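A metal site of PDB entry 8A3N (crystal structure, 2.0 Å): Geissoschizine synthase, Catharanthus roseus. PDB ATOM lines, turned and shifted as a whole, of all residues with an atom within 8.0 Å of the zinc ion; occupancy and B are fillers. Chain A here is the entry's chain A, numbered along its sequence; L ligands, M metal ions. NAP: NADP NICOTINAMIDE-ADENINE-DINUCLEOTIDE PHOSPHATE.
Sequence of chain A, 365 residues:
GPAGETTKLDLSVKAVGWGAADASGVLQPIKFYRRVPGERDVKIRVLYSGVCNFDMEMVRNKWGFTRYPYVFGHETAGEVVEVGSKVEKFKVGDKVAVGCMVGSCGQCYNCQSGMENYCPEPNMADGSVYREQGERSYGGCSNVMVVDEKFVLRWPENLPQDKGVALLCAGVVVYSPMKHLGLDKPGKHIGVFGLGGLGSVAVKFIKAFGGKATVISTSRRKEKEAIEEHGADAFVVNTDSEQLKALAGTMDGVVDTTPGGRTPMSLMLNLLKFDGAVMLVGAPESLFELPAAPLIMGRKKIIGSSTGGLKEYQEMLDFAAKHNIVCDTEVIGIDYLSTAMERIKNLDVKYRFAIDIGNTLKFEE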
ATOM      1  N   GLY A  50      -2.504  29.319 -22.482  1.00  0.00           N
ATOM      2  CA  GLY A  50      -1.340  29.040 -21.664  1.00  0.00           C
ATOM      3  C   GLY A  50      -0.064  29.042 -22.515  1.00  0.00           C
ATOM      4  O   GLY A  50      -0.120  28.816 -23.718  1.00  0.00           O
ATOM      5  N   VAL A  51       1.061  29.348 -21.879  1.00  0.00           N
ATOM      6  CA  VAL A  51       2.357  29.190 -22.526  1.00  0.00           C
ATOM      7  C   VAL A  51       3.279  28.496 -21.512  1.00  0.00           C
ATOM      8  O   VAL A  51       3.144  28.720 -20.313  1.00  0.00           O
ATOM      9  CB  VAL A  51       2.906  30.532 -23.052  1.00  0.00           C
ATOM     10  CG1 VAL A  51       2.986  31.600 -21.984  1.00  0.00           C
ATOM     11  CG2 VAL A  51       4.251  30.379 -23.749  1.00  0.00           C
ATOM     12  N   CYS A  52       4.158  27.620 -21.985  1.00  0.00           N
ATOM     13  CA  CYS A  52       4.992  26.824 -21.108  1.00  0.00           C
ATOM     14  C   CYS A  52       6.337  26.524 -21.770  1.00  0.00           C
ATOM     15  O   CYS A  52       6.602  26.984 -22.875  1.00  0.00           O
ATOM     16  CB  CYS A  52       4.295  25.532 -20.719  1.00  0.00           C
ATOM     17  SG  CYS A  52       4.258  24.301 -22.044  1.00  0.00           S
ATOM     18  N   ASN A  53       7.184  25.799 -21.038  1.00  0.00           N
ATOM     19  CA  ASN A  53       8.513  25.400 -21.467  1.00  0.00           C
ATOM     20  C   ASN A  53       8.494  24.782 -22.856  1.00  0.00           C
ATOM     21  O   ASN A  53       9.362  25.089 -23.672  1.00  0.00           O
ATOM     22  CB  ASN A  53       9.126  24.467 -20.406  1.00  0.00           C
ATOM     23  CG  ASN A  53      10.372  23.763 -20.878  1.00  0.00           C
ATOM     24  OD1 ASN A  53      10.295  22.678 -21.473  1.00  0.00           O
ATOM     25  ND2 ASN A  53      11.518  24.341 -20.589  1.00  0.00           N
ATOM     26  N   PHE A  54       7.507  23.909 -23.118  1.00  0.00           N
ATOM     27  CA  PHE A  54       7.408  23.231 -24.399  1.00  0.00           C
ATOM     28  C   PHE A  54       7.321  24.242 -25.538  1.00  0.00           C
ATOM     29  O   PHE A  54       8.040  24.113 -26.522  1.00  0.00           O
ATOM     30  CB  PHE A  54       6.203  22.289 -24.414  1.00  0.00           C
ATOM     31  CG  PHE A  54       6.002  21.561 -25.716  1.00  0.00           C
ATOM     32  CD1 PHE A  54       6.758  20.444 -26.024  1.00  0.00           C
ATOM     33  CD2 PHE A  54       5.071  22.001 -26.652  1.00  0.00           C
ATOM     34  CE1 PHE A  54       6.576  19.770 -27.226  1.00  0.00           C
ATOM     35  CE2 PHE A  54       4.888  21.328 -27.853  1.00  0.00           C
ATOM     36  CZ  PHE A  54       5.654  20.215 -28.142  1.00  0.00           C
ATOM     37  N   ASP A  55       6.453  25.250 -25.383  1.00  0.00           N
ATOM     38  CA  ASP A  55       6.246  26.265 -26.404  1.00  0.00           C
ATOM     39  C   ASP A  55       7.508  27.081 -26.600  1.00  0.00           C
ATOM     40  O   ASP A  55       7.869  27.427 -27.714  1.00  0.00           O
ATOM     41  CB  ASP A  55       5.119  27.234 -26.041  1.00  0.00           C
ATOM     42  CG  ASP A  55       3.792  26.534 -25.820  1.00  0.00           C
ATOM     43  OD1 ASP A  55       3.409  25.727 -26.707  1.00  0.00           O
ATOM     44  OD2 ASP A  55       3.168  26.788 -24.768  1.00  0.00           O
ATOM     45  N   GLY A  73       0.444  26.747 -29.187  1.00  0.00           N
ATOM     46  CA  GLY A  73      -0.690  26.815 -28.278  1.00  0.00           C
ATOM     47  C   GLY A  73      -1.388  25.466 -28.159  1.00  0.00           C
ATOM     48  O   GLY A  73      -2.174  25.096 -29.039  1.00  0.00           O
ATOM     49  N   HIS A  74      -1.101  24.768 -27.052  1.00  0.00           N
ATOM     50  CA  HIS A  74      -1.731  23.494 -26.725  1.00  0.00           C
ATOM     51  C   HIS A  74      -2.531  23.614 -25.436  1.00  0.00           C
ATOM     52  O   HIS A  74      -2.945  22.615 -24.861  1.00  0.00           O
ATOM     53  CB  HIS A  74      -0.662  22.404 -26.592  1.00  0.00           C
ATOM     54  CG  HIS A  74       0.412  22.739 -25.599  1.00  0.00           C
ATOM     55  ND1 HIS A  74       1.548  23.419 -25.941  1.00  0.00           N
ATOM     56  CD2 HIS A  74       0.489  22.455 -24.268  1.00  0.00           C
ATOM     57  CE1 HIS A  74       2.309  23.564 -24.860  1.00  0.00           C
ATOM     58  NE2 HIS A  74       1.654  22.999 -23.813  1.00  0.00           N
ATOM     59  N   GLU A  75      -2.740  24.854 -24.963  1.00  0.00           N
ATOM     60  CA  GLU A  75      -3.431  25.120 -23.719  1.00  0.00           C
ATOM     61  C   GLU A  75      -4.448  26.216 -23.975  1.00  0.00           C
ATOM     62  O   GLU A  75      -4.206  27.356 -23.599  1.00  0.00           O
ATOM     63  CB  GLU A  75      -2.472  25.589 -22.626  1.00  0.00           C
ATOM     64  CG  GLU A  75      -1.250  24.718 -22.399  1.00  0.00           C
ATOM     65  CD  GLU A  75      -0.317  25.217 -21.295  1.00  0.00           C
ATOM     66  OE1 GLU A  75      -0.738  26.088 -20.518  1.00  0.00           O
ATOM     67  OE2 GLU A  75       0.821  24.766 -21.241  1.00  0.00           O
ATOM     68  N   CYS A 100      -3.732  19.475 -26.754  1.00  0.00           N
ATOM     69  CA  CYS A 100      -2.588  19.400 -27.656  1.00  0.00           C
ATOM     70  C   CYS A 100      -3.007  18.863 -29.023  1.00  0.00           C
ATOM     71  O   CYS A 100      -2.311  19.103 -29.995  1.00  0.00           O
ATOM     72  CB  CYS A 100      -1.450  18.579 -27.061  1.00  0.00           C
ATOM     73  SG  CYS A 100      -1.825  16.827 -26.801  1.00  0.00           S
ATOM     74  N   VAL A 165      -6.296  27.388 -17.202  1.00  0.00           N
ATOM     75  CA  VAL A 165      -5.958  26.946 -18.554  1.00  0.00           C
ATOM     76  C   VAL A 165      -4.685  26.087 -18.542  1.00  0.00           C
ATOM     77  O   VAL A 165      -4.566  25.146 -19.335  1.00  0.00           O
ATOM     78  CB  VAL A 165      -5.868  28.131 -19.550  1.00  0.00           C
ATOM     79  CG1 VAL A 165      -4.740  29.110 -19.232  1.00  0.00           C
ATOM     80  CG2 VAL A 165      -5.787  27.640 -20.975  1.00  0.00           C
ATOM     81  N   ALA A 166      -3.766  26.349 -17.605  1.00  0.00           N
ATOM     82  CA  ALA A 166      -2.532  25.584 -17.484  1.00  0.00           C
ATOM     83  C   ALA A 166      -2.790  24.121 -17.079  1.00  0.00           C
ATOM     84  O   ALA A 166      -1.934  23.285 -17.323  1.00  0.00           O
ATOM     85  CB  ALA A 166      -1.593  26.245 -16.506  1.00  0.00           C
ATOM     86  N   LEU A 168      -4.554  22.173 -18.575  1.00  0.00           N
ATOM     87  CA  LEU A 168      -4.621  21.434 -19.822  1.00  0.00           C
ATOM     88  C   LEU A 168      -3.276  20.813 -20.162  1.00  0.00           C
ATOM     89  O   LEU A 168      -3.197  19.926 -20.999  1.00  0.00           O
ATOM     90  CB  LEU A 168      -5.044  22.397 -20.935  1.00  0.00           C
ATOM     91  CG  LEU A 168      -6.481  22.900 -20.827  1.00  0.00           C
ATOM     92  CD1 LEU A 168      -6.748  23.971 -21.878  1.00  0.00           C
ATOM     93  CD2 LEU A 168      -7.451  21.742 -20.981  1.00  0.00           C
ATOM     94  N   CYS A 169      -2.222  21.301 -19.509  1.00  0.00           N
ATOM     95  CA  CYS A 169      -0.872  20.815 -19.731  1.00  0.00           C
ATOM     96  C   CYS A 169      -0.335  20.226 -18.425  1.00  0.00           C
ATOM     97  O   CYS A 169      -0.087  19.027 -18.359  1.00  0.00           O
ATOM     98  CB  CYS A 169      -0.044  21.985 -20.231  1.00  0.00           C
ATOM     99  SG  CYS A 169       1.721  21.639 -20.466  1.00  0.00           S
ATOM    100  N   ALA A 170      -0.221  21.066 -17.396  1.00  0.00           N
ATOM    101  CA  ALA A 170       0.271  20.666 -16.086  1.00  0.00           C
ATOM    102  C   ALA A 170      -0.581  19.532 -15.502  1.00  0.00           C
ATOM    103  O   ALA A 170      -0.036  18.576 -14.951  1.00  0.00           O
ATOM    104  CB  ALA A 170       0.267  21.862 -15.164  1.00  0.00           C
ATOM    105  N   VAL A 173      -0.890  15.851 -17.800  1.00  0.00           N
ATOM    106  CA  VAL A 173       0.355  15.117 -17.944  1.00  0.00           C
ATOM    107  C   VAL A 173       0.617  14.259 -16.697  1.00  0.00           C
ATOM    108  O   VAL A 173       1.151  13.164 -16.813  1.00  0.00           O
ATOM    109  CB  VAL A 173       1.542  16.052 -18.238  1.00  0.00           C
ATOM    110  CG1 VAL A 173       2.878  15.305 -18.186  1.00  0.00           C
ATOM    111  CG2 VAL A 173       1.401  16.782 -19.575  1.00  0.00           C
ATOM    112  N   LEU A 198       3.943  21.367 -13.511  1.00  0.00           N
ATOM    113  CA  LEU A 198       3.556  19.960 -13.392  1.00  0.00           C
ATOM    114  C   LEU A 198       3.673  19.508 -11.935  1.00  0.00           C
ATOM    115  O   LEU A 198       2.740  18.908 -11.400  1.00  0.00           O
ATOM    116  CB  LEU A 198       4.441  19.090 -14.280  1.00  0.00           C
ATOM    117  CG  LEU A 198       3.890  18.792 -15.669  1.00  0.00           C
ATOM    118  CD1 LEU A 198       3.928  20.031 -16.551  1.00  0.00           C
ATOM    119  CD2 LEU A 198       4.659  17.647 -16.307  1.00  0.00           C
ATOM    120  N   THR A 307       0.975  13.574 -22.371  1.00  0.00           N
ATOM    121  CA  THR A 307      -0.344  14.151 -22.210  1.00  0.00           C
ATOM    122  C   THR A 307      -1.348  13.104 -21.735  1.00  0.00           C
ATOM    123  O   THR A 307      -1.109  12.421 -20.730  1.00  0.00           O
ATOM    124  CB  THR A 307      -0.753  14.930 -23.474  1.00  0.00           C
ATOM    125  OG1 THR A 307      -0.957  13.996 -24.545  1.00  0.00           O
ATOM    126  CG2 THR A 307       0.286  15.950 -23.899  1.00  0.00           C
ATOM    127  N   ARG A 352       3.358  29.400 -14.213  1.00  0.00           N
ATOM    128  CA  ARG A 352       2.963  29.432 -15.612  1.00  0.00           C
ATOM    129  C   ARG A 352       2.430  30.819 -15.949  1.00  0.00           C
ATOM    130  O   ARG A 352       1.884  31.504 -15.090  1.00  0.00           O
ATOM    131  CB  ARG A 352       1.874  28.400 -15.895  1.00  0.00           C
ATOM    132  CG  ARG A 352       2.340  26.953 -15.836  1.00  0.00           C
ATOM    133  CD  ARG A 352       3.335  26.613 -16.915  1.00  0.00           C
ATOM    134  NE  ARG A 352       3.582  25.190 -16.964  1.00  0.00           N
ATOM    135  CZ  ARG A 352       2.910  24.332 -17.711  1.00  0.00           C
ATOM    136  NH1 ARG A 352       1.808  24.715 -18.324  1.00  0.00           N
ATOM    137  NH2 ARG A 352       3.325  23.076 -17.823  1.00  0.00           N
HETATM  138  PA  NAP L   1       9.522  24.157 -15.920  1.00  0.00           P
HETATM  139  O1A NAP L   1      10.421  24.604 -17.006  1.00  0.00           O
HETATM  140  O2A NAP L   1       8.663  25.167 -15.238  1.00  0.00           O
HETATM  141  O5B NAP L   1      10.379  23.371 -14.838  1.00  0.00           O
HETATM  142  C5B NAP L   1       9.674  22.765 -13.747  1.00  0.00           C
HETATM  143  C4B NAP L   1      10.624  22.568 -12.602  1.00  0.00           C
HETATM  144  O4B NAP L   1      11.616  21.571 -12.976  1.00  0.00           O
HETATM  145  C3B NAP L   1      11.484  23.777 -12.199  1.00  0.00           C
HETATM  146  O3B NAP L   1      10.764  24.683 -11.378  1.00  0.00           O
HETATM  147  C2B NAP L   1      12.575  23.051 -11.411  1.00  0.00           C
HETATM  148  O2B NAP L   1      12.000  22.665 -10.179  1.00  0.00           O
HETATM  149  C1B NAP L   1      12.809  21.815 -12.272  1.00  0.00           C
HETATM  150  N9A NAP L   1      13.884  21.962 -13.232  1.00  0.00           N
HETATM  151  C8A NAP L   1      13.890  22.738 -14.371  1.00  0.00           C
HETATM  152  N7A NAP L   1      15.019  22.673 -15.030  1.00  0.00           N
HETATM  153  C5A NAP L   1      15.803  21.808 -14.280  1.00  0.00           C
HETATM  154  C6A NAP L   1      17.103  21.306 -14.465  1.00  0.00           C
HETATM  155  N6A NAP L   1      17.871  21.658 -15.491  1.00  0.00           N
HETATM  156  N1A NAP L   1      17.585  20.447 -13.540  1.00  0.00           N
HETATM  157  C2A NAP L   1      16.807  20.126 -12.495  1.00  0.00           C
HETATM  158  N3A NAP L   1      15.557  20.516 -12.228  1.00  0.00           N
HETATM  159  C4A NAP L   1      15.112  21.363 -13.172  1.00  0.00           C
HETATM  160  O3  NAP L   1       8.604  22.933 -16.429  1.00  0.00           O
HETATM  161  PN  NAP L   1       7.068  22.458 -16.321  1.00  0.00           P
HETATM  162  O1N NAP L   1       6.697  22.188 -14.901  1.00  0.00           O
HETATM  163  O2N NAP L   1       6.214  23.363 -17.143  1.00  0.00           O
HETATM  164  O5D NAP L   1       7.174  21.050 -17.107  1.00  0.00           O
HETATM  165  C5D NAP L   1       7.982  19.996 -16.543  1.00  0.00           C
HETATM  166  C4D NAP L   1       8.581  19.153 -17.640  1.00  0.00           C
HETATM  167  O4D NAP L   1       7.541  18.426 -18.331  1.00  0.00           O
HETATM  168  C3D NAP L   1       9.342  19.915 -18.732  1.00  0.00           C
HETATM  169  O3D NAP L   1      10.525  19.211 -19.088  1.00  0.00           O
HETATM  170  C2D NAP L   1       8.319  20.004 -19.873  1.00  0.00           C
HETATM  171  O2D NAP L   1       8.879  20.209 -21.157  1.00  0.00           O
HETATM  172  C1D NAP L   1       7.708  18.605 -19.729  1.00  0.00           C
HETATM  173  N1N NAP L   1       6.405  18.363 -20.390  1.00  0.00           N
HETATM  174  C2N NAP L   1       6.031  17.062 -20.605  1.00  0.00           C
HETATM  175  C3N NAP L   1       4.827  16.761 -21.225  1.00  0.00           C
HETATM  176  C7N NAP L   1       4.454  15.325 -21.424  1.00  0.00           C
HETATM  177  O7N NAP L   1       3.402  15.052 -22.016  1.00  0.00           O
HETATM  178  N7N NAP L   1       5.230  14.382 -20.916  1.00  0.00           N
HETATM  179  C4N NAP L   1       3.989  17.802 -21.619  1.00  0.00           C
HETATM  180  C5N NAP L   1       4.371  19.109 -21.394  1.00  0.00           C
HETATM  181  C6N NAP L   1       5.572  19.388 -20.778  1.00  0.00           C
HETATM  182  P2B NAP L   1      12.775  23.115  -8.846  1.00  0.00           P
HETATM  183  O1X NAP L   1      11.888  22.575  -7.759  1.00  0.00           O
HETATM  184  O2X NAP L   1      12.852  24.645  -8.830  1.00  0.00           O
HETATM  185  O3X NAP L   1      14.138  22.464  -8.874  1.00  0.00           O
HETATM  186 ZN    ZN M   1       2.110  23.398 -21.929  1.00  0.00          ZN
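N of Leu 198 lies within hydrogen-bond range of O1N of the ligand (3.2 Å).
The guanidinium group (NH2) of Arg 352 is in salt-bridge range of an oxygen (O2N) of the ligand (3.0 Å).
The backbone NH (N) of Thr 307 sits at hydrogen-bond distance from an oxygen (O7N) of the ligand (2.9 Å).
OD1 of Asn 53 lies within hydrogen-bond range of O2D of the ligand (2.9 Å).
The side-chain carboxylate (OD2) of Asp 55 is in hydrogen-bond range of the backbone NH (N) of Cys 52, at 3.1 Å.
SG of Cys 169 lies close to NH2 of Arg 352 (3.4 Å).
The side-chain carboxylate (OE1) of Glu 75 lies within salt-bridge range of the guanidinium group (NH1) of Arg 352, 3.6 Å away.
The side-chain sulfur of Cys 52 sits close to the backbone NH of Phe 54 (3.4 Å).
A ring nitrogen (ND1) of His 74 sits close to the side-chain carboxylate (OD1) of Asp 55, 3.1 Å away.
N of Gly 50 sits at hydrogen-bond distance from O of Glu 75 (2.8 Å).
Arg 352 touches the zinc ion (NH1 to ZN, 3.8 Å).
Within 4 Å of the zinc ion: Cys 52, His 74, Glu 75, Cys 169 and Arg 352.
The zinc ion is bound by a ring nitrogen (NE2) of His 74 (2.0 Å).
The zinc ion is bound by OE2 of Glu 75 (2.0 Å).
The zinc ion is bound by SG of Cys 169.
The side-chain sulfur (SG) of Cys 52 binds the zinc ion (2.3 Å).
The zinc ion has four donor atoms within binding distance.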
